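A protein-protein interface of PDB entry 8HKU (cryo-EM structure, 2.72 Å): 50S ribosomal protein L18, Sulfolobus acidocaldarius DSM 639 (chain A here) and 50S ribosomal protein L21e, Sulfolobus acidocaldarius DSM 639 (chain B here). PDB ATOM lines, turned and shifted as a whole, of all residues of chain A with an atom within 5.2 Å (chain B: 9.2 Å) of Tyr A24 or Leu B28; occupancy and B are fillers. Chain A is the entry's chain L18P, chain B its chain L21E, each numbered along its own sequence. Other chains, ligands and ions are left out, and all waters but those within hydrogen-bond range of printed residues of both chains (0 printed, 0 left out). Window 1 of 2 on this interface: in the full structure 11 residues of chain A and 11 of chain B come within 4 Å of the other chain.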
ATOM      1  N   TYR A  20      23.263 -17.899  -9.461  1.00  0.00           N
ATOM      2  CA  TYR A  20      22.245 -16.862  -9.483  1.00  0.00           C
ATOM      3  C   TYR A  20      21.013 -17.248 -10.281  1.00  0.00           C
ATOM      4  O   TYR A  20      19.999 -16.555 -10.188  1.00  0.00           O
ATOM      5  CB  TYR A  20      22.835 -15.568 -10.035  1.00  0.00           C
ATOM      6  CG  TYR A  20      23.637 -14.810  -9.015  1.00  0.00           C
ATOM      7  CD1 TYR A  20      23.016 -13.991  -8.101  1.00  0.00           C
ATOM      8  CD2 TYR A  20      25.008 -14.932  -8.956  1.00  0.00           C
ATOM      9  CE1 TYR A  20      23.731 -13.314  -7.161  1.00  0.00           C
ATOM     10  CE2 TYR A  20      25.735 -14.248  -8.022  1.00  0.00           C
ATOM     11  CZ  TYR A  20      25.090 -13.443  -7.126  1.00  0.00           C
ATOM     12  OH  TYR A  20      25.809 -12.755  -6.188  1.00  0.00           O
ATOM     13  N   TYR A  21      21.075 -18.320 -11.066  1.00  0.00           N
ATOM     14  CA  TYR A  21      19.884 -18.784 -11.762  1.00  0.00           C
ATOM     15  C   TYR A  21      18.908 -19.441 -10.801  1.00  0.00           C
ATOM     16  O   TYR A  21      17.695 -19.250 -10.916  1.00  0.00           O
ATOM     17  CB  TYR A  21      20.285 -19.736 -12.874  1.00  0.00           C
ATOM     18  CG  TYR A  21      21.162 -19.071 -13.888  1.00  0.00           C
ATOM     19  CD1 TYR A  21      20.624 -18.254 -14.860  1.00  0.00           C
ATOM     20  CD2 TYR A  21      22.532 -19.239 -13.862  1.00  0.00           C
ATOM     21  CE1 TYR A  21      21.420 -17.634 -15.783  1.00  0.00           C
ATOM     22  CE2 TYR A  21      23.338 -18.626 -14.784  1.00  0.00           C
ATOM     23  CZ  TYR A  21      22.776 -17.823 -15.742  1.00  0.00           C
ATOM     24  OH  TYR A  21      23.573 -17.203 -16.668  1.00  0.00           O
ATOM     25  N   THR A  22      19.418 -20.213  -9.844  1.00  0.00           N
ATOM     26  CA  THR A  22      18.567 -20.763  -8.796  1.00  0.00           C
ATOM     27  C   THR A  22      18.151 -19.689  -7.803  1.00  0.00           C
ATOM     28  O   THR A  22      17.007 -19.680  -7.340  1.00  0.00           O
ATOM     29  CB  THR A  22      19.292 -21.895  -8.075  1.00  0.00           C
ATOM     30  OG1 THR A  22      19.812 -22.815  -9.038  1.00  0.00           O
ATOM     31  CG2 THR A  22      18.352 -22.625  -7.163  1.00  0.00           C
ATOM     32  N   ARG A  23      19.064 -18.779  -7.461  1.00  0.00           N
ATOM     33  CA  ARG A  23      18.734 -17.716  -6.519  1.00  0.00           C
ATOM     34  C   ARG A  23      17.643 -16.809  -7.060  1.00  0.00           C
ATOM     35  O   ARG A  23      16.858 -16.251  -6.291  1.00  0.00           O
ATOM     36  CB  ARG A  23      19.983 -16.906  -6.187  1.00  0.00           C
ATOM     37  CG  ARG A  23      19.760 -15.846  -5.138  1.00  0.00           C
ATOM     38  CD  ARG A  23      21.035 -15.143  -4.754  1.00  0.00           C
ATOM     39  NE  ARG A  23      20.754 -14.050  -3.837  1.00  0.00           N
ATOM     40  CZ  ARG A  23      20.520 -14.202  -2.543  1.00  0.00           C
ATOM     41  NH1 ARG A  23      20.593 -15.384  -1.965  1.00  0.00           N
ATOM     42  NH2 ARG A  23      20.206 -13.140  -1.811  1.00  0.00           N
ATOM     43  N   TYR A  24      17.582 -16.649  -8.379  1.00  0.00           N
ATOM     44  CA  TYR A  24      16.514 -15.873  -8.991  1.00  0.00           C
ATOM     45  C   TYR A  24      15.150 -16.484  -8.699  1.00  0.00           C
ATOM     46  O   TYR A  24      14.191 -15.766  -8.403  1.00  0.00           O
ATOM     47  CB  TYR A  24      16.773 -15.774 -10.493  1.00  0.00           C
ATOM     48  CG  TYR A  24      15.739 -15.020 -11.283  1.00  0.00           C
ATOM     49  CD1 TYR A  24      15.081 -13.931 -10.749  1.00  0.00           C
ATOM     50  CD2 TYR A  24      15.421 -15.402 -12.568  1.00  0.00           C
ATOM     51  CE1 TYR A  24      14.136 -13.255 -11.470  1.00  0.00           C
ATOM     52  CE2 TYR A  24      14.482 -14.729 -13.295  1.00  0.00           C
ATOM     53  CZ  TYR A  24      13.841 -13.657 -12.742  1.00  0.00           C
ATOM     54  OH  TYR A  24      12.895 -12.985 -13.471  1.00  0.00           O
ATOM     55  N   THR A  25      15.045 -17.813  -8.760  1.00  0.00           N
ATOM     56  CA  THR A  25      13.771 -18.479  -8.511  1.00  0.00           C
ATOM     57  C   THR A  25      13.309 -18.311  -7.069  1.00  0.00           C
ATOM     58  O   THR A  25      12.113 -18.159  -6.813  1.00  0.00           O
ATOM     59  CB  THR A  25      13.874 -19.956  -8.862  1.00  0.00           C
ATOM     60  OG1 THR A  25      14.429 -20.097 -10.170  1.00  0.00           O
ATOM     61  CG2 THR A  25      12.513 -20.594  -8.843  1.00  0.00           C
ATOM     62  N   TYR A  26      14.232 -18.360  -6.108  1.00  0.00           N
ATOM     63  CA  TYR A  26      13.841 -18.188  -4.712  1.00  0.00           C
ATOM     64  C   TYR A  26      13.248 -16.810  -4.467  1.00  0.00           C
ATOM     65  O   TYR A  26      12.242 -16.677  -3.766  1.00  0.00           O
ATOM     66  CB  TYR A  26      15.040 -18.402  -3.790  1.00  0.00           C
ATOM     67  CG  TYR A  26      15.581 -19.804  -3.780  1.00  0.00           C
ATOM     68  CD1 TYR A  26      14.745 -20.888  -3.600  1.00  0.00           C
ATOM     69  CD2 TYR A  26      16.932 -20.041  -3.944  1.00  0.00           C
ATOM     70  CE1 TYR A  26      15.242 -22.166  -3.593  1.00  0.00           C
ATOM     71  CE2 TYR A  26      17.434 -21.312  -3.941  1.00  0.00           C
ATOM     72  CZ  TYR A  26      16.586 -22.370  -3.764  1.00  0.00           C
ATOM     73  OH  TYR A  26      17.082 -23.645  -3.761  1.00  0.00           O
ATOM     74  N   VAL A  27      13.866 -15.770  -5.028  1.00  0.00           N
ATOM     75  CA  VAL A  27      13.447 -14.402  -4.740  1.00  0.00           C
ATOM     76  C   VAL A  27      12.070 -14.120  -5.325  1.00  0.00           C
ATOM     77  O   VAL A  27      11.246 -13.441  -4.703  1.00  0.00           O
ATOM     78  CB  VAL A  27      14.498 -13.407  -5.259  1.00  0.00           C
ATOM     79  CG1 VAL A  27      14.080 -11.998  -4.947  1.00  0.00           C
ATOM     80  CG2 VAL A  27      15.840 -13.698  -4.647  1.00  0.00           C
ATOM     81  N   ILE A  28      11.796 -14.633  -6.526  1.00  0.00           N
ATOM     82  CA  ILE A  28      10.473 -14.469  -7.123  1.00  0.00           C
ATOM     83  C   ILE A  28       9.407 -15.089  -6.239  1.00  0.00           C
ATOM     84  O   ILE A  28       8.318 -14.531  -6.067  1.00  0.00           O
ATOM     85  CB  ILE A  28      10.444 -15.071  -8.538  1.00  0.00           C
ATOM     86  CG1 ILE A  28      11.472 -14.394  -9.427  1.00  0.00           C
ATOM     87  CG2 ILE A  28       9.074 -14.936  -9.139  1.00  0.00           C
ATOM     88  CD1 ILE A  28      11.190 -12.935  -9.641  1.00  0.00           C
ATOM     89  N   GLY B  23      22.743  -9.401 -19.758  1.00  0.00           N
ATOM     90  CA  GLY B  23      22.763 -10.640 -19.014  1.00  0.00           C
ATOM     91  C   GLY B  23      21.437 -10.909 -18.328  1.00  0.00           C
ATOM     92  O   GLY B  23      20.643 -10.007 -18.058  1.00  0.00           O
ATOM     93  N   ALA B  24      21.210 -12.187 -18.028  1.00  0.00           N
ATOM     94  CA  ALA B  24      19.981 -12.600 -17.360  1.00  0.00           C
ATOM     95  C   ALA B  24      19.897 -11.980 -15.969  1.00  0.00           C
ATOM     96  O   ALA B  24      20.894 -11.876 -15.252  1.00  0.00           O
ATOM     97  CB  ALA B  24      19.910 -14.118 -17.280  1.00  0.00           C
ATOM     98  N   ILE B  25      18.672 -11.645 -15.563  1.00  0.00           N
ATOM     99  CA  ILE B  25      18.378 -10.470 -14.737  1.00  0.00           C
ATOM    100  C   ILE B  25      19.443 -10.189 -13.687  1.00  0.00           C
ATOM    101  O   ILE B  25      19.772 -11.060 -12.872  1.00  0.00           O
ATOM    102  CB  ILE B  25      17.002 -10.583 -14.069  1.00  0.00           C
ATOM    103  CG1 ILE B  25      16.833  -9.457 -13.061  1.00  0.00           C
ATOM    104  CG2 ILE B  25      16.836 -11.915 -13.414  1.00  0.00           C
ATOM    105  CD1 ILE B  25      15.417  -9.265 -12.652  1.00  0.00           C
ATOM    106  N   PRO B  26      20.043  -9.005 -13.721  1.00  0.00           N
ATOM    107  CA  PRO B  26      21.075  -8.657 -12.739  1.00  0.00           C
ATOM    108  C   PRO B  26      20.555  -8.253 -11.364  1.00  0.00           C
ATOM    109  O   PRO B  26      21.116  -8.679 -10.349  1.00  0.00           O
ATOM    110  CB  PRO B  26      21.817  -7.494 -13.415  1.00  0.00           C
ATOM    111  CG  PRO B  26      20.827  -6.883 -14.322  1.00  0.00           C
ATOM    112  CD  PRO B  26      19.904  -7.982 -14.772  1.00  0.00           C
ATOM    113  N   LYS B  27      19.506  -7.432 -11.300  1.00  0.00           N
ATOM    114  CA  LYS B  27      19.114  -6.789 -10.050  1.00  0.00           C
ATOM    115  C   LYS B  27      18.014  -7.587  -9.373  1.00  0.00           C
ATOM    116  O   LYS B  27      16.864  -7.571  -9.815  1.00  0.00           O
ATOM    117  CB  LYS B  27      18.677  -5.345 -10.276  1.00  0.00           C
ATOM    118  CG  LYS B  27      19.817  -4.436 -10.682  1.00  0.00           C
ATOM    119  CD  LYS B  27      19.333  -3.033 -10.957  1.00  0.00           C
ATOM    120  CE  LYS B  27      18.921  -2.362  -9.654  1.00  0.00           C
ATOM    121  NZ  LYS B  27      20.076  -2.105  -8.751  1.00  0.00           N
ATOM    122  N   LEU B  28      18.372  -8.263  -8.284  1.00  0.00           N
ATOM    123  CA  LEU B  28      17.418  -9.016  -7.490  1.00  0.00           C
ATOM    124  C   LEU B  28      16.874  -8.228  -6.313  1.00  0.00           C
ATOM    125  O   LEU B  28      15.819  -8.588  -5.787  1.00  0.00           O
ATOM    126  CB  LEU B  28      18.058 -10.309  -6.979  1.00  0.00           C
ATOM    127  CG  LEU B  28      18.638 -11.271  -8.017  1.00  0.00           C
ATOM    128  CD1 LEU B  28      19.350 -12.421  -7.348  1.00  0.00           C
ATOM    129  CD2 LEU B  28      17.559 -11.793  -8.937  1.00  0.00           C
ATOM    130  N   SER B  29      17.555  -7.160  -5.893  1.00  0.00           N
ATOM    131  CA  SER B  29      17.109  -6.415  -4.721  1.00  0.00           C
ATOM    132  C   SER B  29      15.822  -5.648  -4.975  1.00  0.00           C
ATOM    133  O   SER B  29      15.119  -5.309  -4.019  1.00  0.00           O
ATOM    134  CB  SER B  29      18.196  -5.452  -4.248  1.00  0.00           C
ATOM    135  OG  SER B  29      18.488  -4.480  -5.229  1.00  0.00           O
ATOM    136  N   LEU B  30      15.502  -5.358  -6.234  1.00  0.00           N
ATOM    137  CA  LEU B  30      14.223  -4.735  -6.538  1.00  0.00           C
ATOM    138  C   LEU B  30      13.082  -5.734  -6.440  1.00  0.00           C
ATOM    139  O   LEU B  30      11.945  -5.349  -6.156  1.00  0.00           O
ATOM    140  CB  LEU B  30      14.265  -4.105  -7.927  1.00  0.00           C
ATOM    141  CG  LEU B  30      15.177  -2.888  -8.076  1.00  0.00           C
ATOM    142  CD1 LEU B  30      15.128  -2.359  -9.491  1.00  0.00           C
ATOM    143  CD2 LEU B  30      14.784  -1.811  -7.094  1.00  0.00           C
ATOM    144  N   LEU B  31      13.371  -7.016  -6.653  1.00  0.00           N
ATOM    145  CA  LEU B  31      12.365  -8.065  -6.603  1.00  0.00           C
ATOM    146  C   LEU B  31      12.035  -8.517  -5.189  1.00  0.00           C
ATOM    147  O   LEU B  31      11.117  -9.321  -5.019  1.00  0.00           O
ATOM    148  CB  LEU B  31      12.833  -9.264  -7.419  1.00  0.00           C
ATOM    149  CG  LEU B  31      13.093  -8.986  -8.894  1.00  0.00           C
ATOM    150  CD1 LEU B  31      13.796 -10.149  -9.532  1.00  0.00           C
ATOM    151  CD2 LEU B  31      11.793  -8.723  -9.591  1.00  0.00           C
ATOM    152  N   MET B  32      12.750  -8.033  -4.181  1.00  0.00           N
ATOM    153  CA  MET B  32      12.511  -8.423  -2.800  1.00  0.00           C
ATOM    154  C   MET B  32      11.451  -7.572  -2.123  1.00  0.00           C
ATOM    155  O   MET B  32      11.156  -7.799  -0.948  1.00  0.00           O
ATOM    156  CB  MET B  32      13.810  -8.354  -1.996  1.00  0.00           C
ATOM    157  CG  MET B  32      15.014  -8.886  -2.734  1.00  0.00           C
ATOM    158  SD  MET B  32      16.488  -8.986  -1.724  1.00  0.00           S
ATOM    159  CE  MET B  32      17.411 -10.246  -2.585  1.00  0.00           C
ATOM    160  N   HIS B  33      10.878  -6.601  -2.822  1.00  0.00           N
ATOM    161  CA  HIS B  33       9.841  -5.747  -2.265  1.00  0.00           C
ATOM    162  C   HIS B  33       8.492  -6.144  -2.844  1.00  0.00           C
ATOM    163  O   HIS B  33       8.371  -6.367  -4.052  1.00  0.00           O
ATOM    164  CB  HIS B  33      10.126  -4.275  -2.556  1.00  0.00           C
ATOM    165  CG  HIS B  33       9.039  -3.353  -2.101  1.00  0.00           C
ATOM    166  ND1 HIS B  33       8.607  -3.302  -0.795  1.00  0.00           N
ATOM    167  CD2 HIS B  33       8.292  -2.453  -2.780  1.00  0.00           C
ATOM    168  CE1 HIS B  33       7.641  -2.409  -0.687  1.00  0.00           C
ATOM    169  NE2 HIS B  33       7.430  -1.879  -1.878  1.00  0.00           N
ATOM    170  N   ASN B  46      12.015  -4.401 -19.422  1.00  0.00           N
ATOM    171  CA  ASN B  46      13.300  -5.079 -19.407  1.00  0.00           C
ATOM    172  C   ASN B  46      13.408  -5.916 -20.671  1.00  0.00           C
ATOM    173  O   ASN B  46      12.691  -6.915 -20.797  1.00  0.00           O
ATOM    174  CB  ASN B  46      13.418  -5.958 -18.167  1.00  0.00           C
ATOM    175  CG  ASN B  46      14.838  -6.359 -17.861  1.00  0.00           C
ATOM    176  OD1 ASN B  46      15.657  -6.513 -18.754  1.00  0.00           O
ATOM    177  ND2 ASN B  46      15.135  -6.528 -16.586  1.00  0.00           N
ATOM    178  N   SER B  48      15.245  -8.194 -21.851  1.00  0.00           N
ATOM    179  CA  SER B  48      15.690  -9.579 -21.825  1.00  0.00           C
ATOM    180  C   SER B  48      14.745 -10.516 -21.085  1.00  0.00           C
ATOM    181  O   SER B  48      14.931 -11.731 -21.161  1.00  0.00           O
ATOM    182  CB  SER B  48      17.087  -9.668 -21.213  1.00  0.00           C
ATOM    183  OG  SER B  48      17.121  -9.057 -19.945  1.00  0.00           O
ATOM    184  N   ILE B  49      13.748  -9.996 -20.381  1.00  0.00           N
ATOM    185  CA  ILE B  49      12.712 -10.806 -19.754  1.00  0.00           C
ATOM    186  C   ILE B  49      11.481 -10.728 -20.646  1.00  0.00           C
ATOM    187  O   ILE B  49      10.834  -9.682 -20.726  1.00  0.00           O
ATOM    188  CB  ILE B  49      12.395 -10.320 -18.334  1.00  0.00           C
ATOM    189  CG1 ILE B  49      13.654 -10.268 -17.474  1.00  0.00           C
ATOM    190  CG2 ILE B  49      11.355 -11.204 -17.692  1.00  0.00           C
ATOM    191  CD1 ILE B  49      14.419 -11.542 -17.444  1.00  0.00           C
ATOM    192  N   HIS B  50      11.125 -11.834 -21.295  1.00  0.00           N
ATOM    193  CA  HIS B  50      10.123 -11.818 -22.353  1.00  0.00           C
ATOM    194  C   HIS B  50       8.735 -12.226 -21.888  1.00  0.00           C
ATOM    195  O   HIS B  50       7.856 -12.424 -22.725  1.00  0.00           O
ATOM    196  CB  HIS B  50      10.552 -12.714 -23.510  1.00  0.00           C
ATOM    197  CG  HIS B  50      11.828 -12.287 -24.160  1.00  0.00           C
ATOM    198  ND1 HIS B  50      12.613 -13.146 -24.893  1.00  0.00           N
ATOM    199  CD2 HIS B  50      12.461 -11.094 -24.176  1.00  0.00           C
ATOM    200  CE1 HIS B  50      13.670 -12.497 -25.343  1.00  0.00           C
ATOM    201  NE2 HIS B  50      13.605 -11.252 -24.916  1.00  0.00           N
ATOM    202  N   LYS B  51       8.508 -12.344 -20.585  1.00  0.00           N
ATOM    203  CA  LYS B  51       7.214 -12.731 -20.045  1.00  0.00           C
ATOM    204  C   LYS B  51       6.578 -11.544 -19.342  1.00  0.00           C
ATOM    205  O   LYS B  51       7.240 -10.860 -18.560  1.00  0.00           O
ATOM    206  CB  LYS B  51       7.356 -13.899 -19.069  1.00  0.00           C
ATOM    207  CG  LYS B  51       7.726 -15.220 -19.710  1.00  0.00           C
ATOM    208  CD  LYS B  51       6.615 -15.716 -20.604  1.00  0.00           C
ATOM    209  CE  LYS B  51       6.948 -17.053 -21.231  1.00  0.00           C
ATOM    210  NZ  LYS B  51       6.733 -18.197 -20.314  1.00  0.00           N
ATOM    211  N   LYS B  71       1.626 -13.820  -9.644  1.00  0.00           N
ATOM    212  CA  LYS B  71       2.861 -13.107  -9.372  1.00  0.00           C
ATOM    213  C   LYS B  71       2.939 -11.757 -10.071  1.00  0.00           C
ATOM    214  O   LYS B  71       3.939 -11.056  -9.918  1.00  0.00           O
ATOM    215  CB  LYS B  71       4.058 -13.963  -9.777  1.00  0.00           C
ATOM    216  CG  LYS B  71       4.362 -15.083  -8.805  1.00  0.00           C
ATOM    217  CD  LYS B  71       5.400 -16.014  -9.374  1.00  0.00           C
ATOM    218  CE  LYS B  71       5.156 -17.427  -8.922  1.00  0.00           C
ATOM    219  NZ  LYS B  71       5.686 -18.405  -9.906  1.00  0.00           N
ATOM    220  N   ARG B  89       4.493  -8.094 -14.815  1.00  0.00           N
ATOM    221  CA  ARG B  89       5.383  -8.836 -13.940  1.00  0.00           C
ATOM    222  C   ARG B  89       6.382  -7.891 -13.276  1.00  0.00           C
ATOM    223  O   ARG B  89       6.807  -6.907 -13.878  1.00  0.00           O
ATOM    224  CB  ARG B  89       6.129  -9.908 -14.720  1.00  0.00           C
ATOM    225  CG  ARG B  89       5.301 -11.124 -15.027  1.00  0.00           C
ATOM    226  CD  ARG B  89       6.167 -12.238 -15.541  1.00  0.00           C
ATOM    227  NE  ARG B  89       6.937 -12.844 -14.465  1.00  0.00           N
ATOM    228  CZ  ARG B  89       7.957 -13.670 -14.642  1.00  0.00           C
ATOM    229  NH1 ARG B  89       8.361 -14.018 -15.852  1.00  0.00           N
ATOM    230  NH2 ARG B  89       8.590 -14.157 -13.580  1.00  0.00           N
ATOM    231  N   PRO B  90       6.796  -8.187 -12.042  1.00  0.00           N
ATOM    232  CA  PRO B  90       7.594  -7.213 -11.280  1.00  0.00           C
ATOM    233  C   PRO B  90       8.968  -6.933 -11.856  1.00  0.00           C
ATOM    234  O   PRO B  90       9.607  -5.968 -11.430  1.00  0.00           O
ATOM    235  CB  PRO B  90       7.692  -7.856  -9.894  1.00  0.00           C
ATOM    236  CG  PRO B  90       7.497  -9.287 -10.138  1.00  0.00           C
ATOM    237  CD  PRO B  90       6.511  -9.389 -11.247  1.00  0.00           C
ATOM    238  N   GLU B  91       9.461  -7.750 -12.785  1.00  0.00           N
ATOM    239  CA  GLU B  91      10.724  -7.450 -13.441  1.00  0.00           C
ATOM    240  C   GLU B  91      10.631  -6.242 -14.353  1.00  0.00           C
ATOM    241  O   GLU B  91      11.665  -5.760 -14.819  1.00  0.00           O
ATOM    242  CB  GLU B  91      11.201  -8.649 -14.251  1.00  0.00           C
ATOM    243  CG  GLU B  91      11.521  -9.859 -13.415  1.00  0.00           C
ATOM    244  CD  GLU B  91      10.370 -10.832 -13.336  1.00  0.00           C
ATOM    245  OE1 GLU B  91       9.283 -10.429 -12.887  1.00  0.00           O
ATOM    246  OE2 GLU B  91      10.557 -12.002 -13.713  1.00  0.00           O
ATOM    247  N   HIS B  92       9.425  -5.756 -14.626  1.00  0.00           N
ATOM    248  CA  HIS B  92       9.192  -4.600 -15.479  1.00  0.00           C
ATOM    249  C   HIS B  92       8.673  -3.409 -14.683  1.00  0.00           C
ATOM    250  O   HIS B  92       7.911  -2.600 -15.204  1.00  0.00           O
ATOM    251  CB  HIS B  92       8.212  -4.947 -16.598  1.00  0.00           C
ATOM    252  CG  HIS B  92       8.647  -6.091 -17.458  1.00  0.00           C
ATOM    253  ND1 HIS B  92       9.655  -5.984 -18.387  1.00  0.00           N
ATOM    254  CD2 HIS B  92       8.210  -7.368 -17.525  1.00  0.00           C
ATOM    255  CE1 HIS B  92       9.821  -7.146 -18.988  1.00  0.00           C
ATOM    256  NE2 HIS B  92       8.954  -8.001 -18.487  1.00  0.00           N
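The side-chain hydroxyl of Tyr A24 is in hydrogen-bond range of the side-chain carboxylate of Glu B91, 2.5 Å away.
OE2 of Glu B91 is in salt-bridge range of NH2 of Arg B89, 2.9 Å away.
Among the printed residues, pairs that only touch across the chains: Tyr A24 with Ile B25, Tyr A24 with Leu B28, Tyr A24 with Leu B31, Val A27 with Leu B28, Val A27 with Leu B31, Val A27 with Met B32, Ile A28 with Leu B31 and Ile A28 with Lys B71.
Tyr A24 touches just these residues of chain B: Ile B25 (3.5 Å), Leu B28 (3.7 Å), Leu B31 (3.7 Å) and Glu B91 (2.5 Å). Of chain A, only Tyr A24 and Val A27 come within 4 Å of Leu B28. No residue of chain B comes within 4 Å of Thr A25. Printed residues of chain A within 4 Å of Met B32: Val A27 (3.9 Å). Of the printed residues of chain B, Val A27 touches Leu B28, Leu B31 and Met B32. Printed residues of chain A within 4 Å of Lys B71: Ile A28 (3.8 Å). Printed residues of chain A within 4 Å of Glu B91: Tyr A24. Pro B26 touches none of the printed residues of chain A. Lys B51 touches none of the printed residues of chain A. The nearest residue of chain A that does not touch Leu B28 is Tyr A20 (4.1 Å). The nearest printed residue of chain A that does not touch Glu B91 is Ile A28 (4.2 Å).
Of the 21 printed residues of chain B, 6 touch a printed residue of chain A. Hydrophobic or aromatic side chains of chain B within 4 Å of the printed part of chain A: Ile B25, Leu B28, Leu B31 and Met B32. Hydrophobic or aromatic side chains of chain A within 4 Å of the printed part of chain B: Tyr A24, Val A27 and Ile A28.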
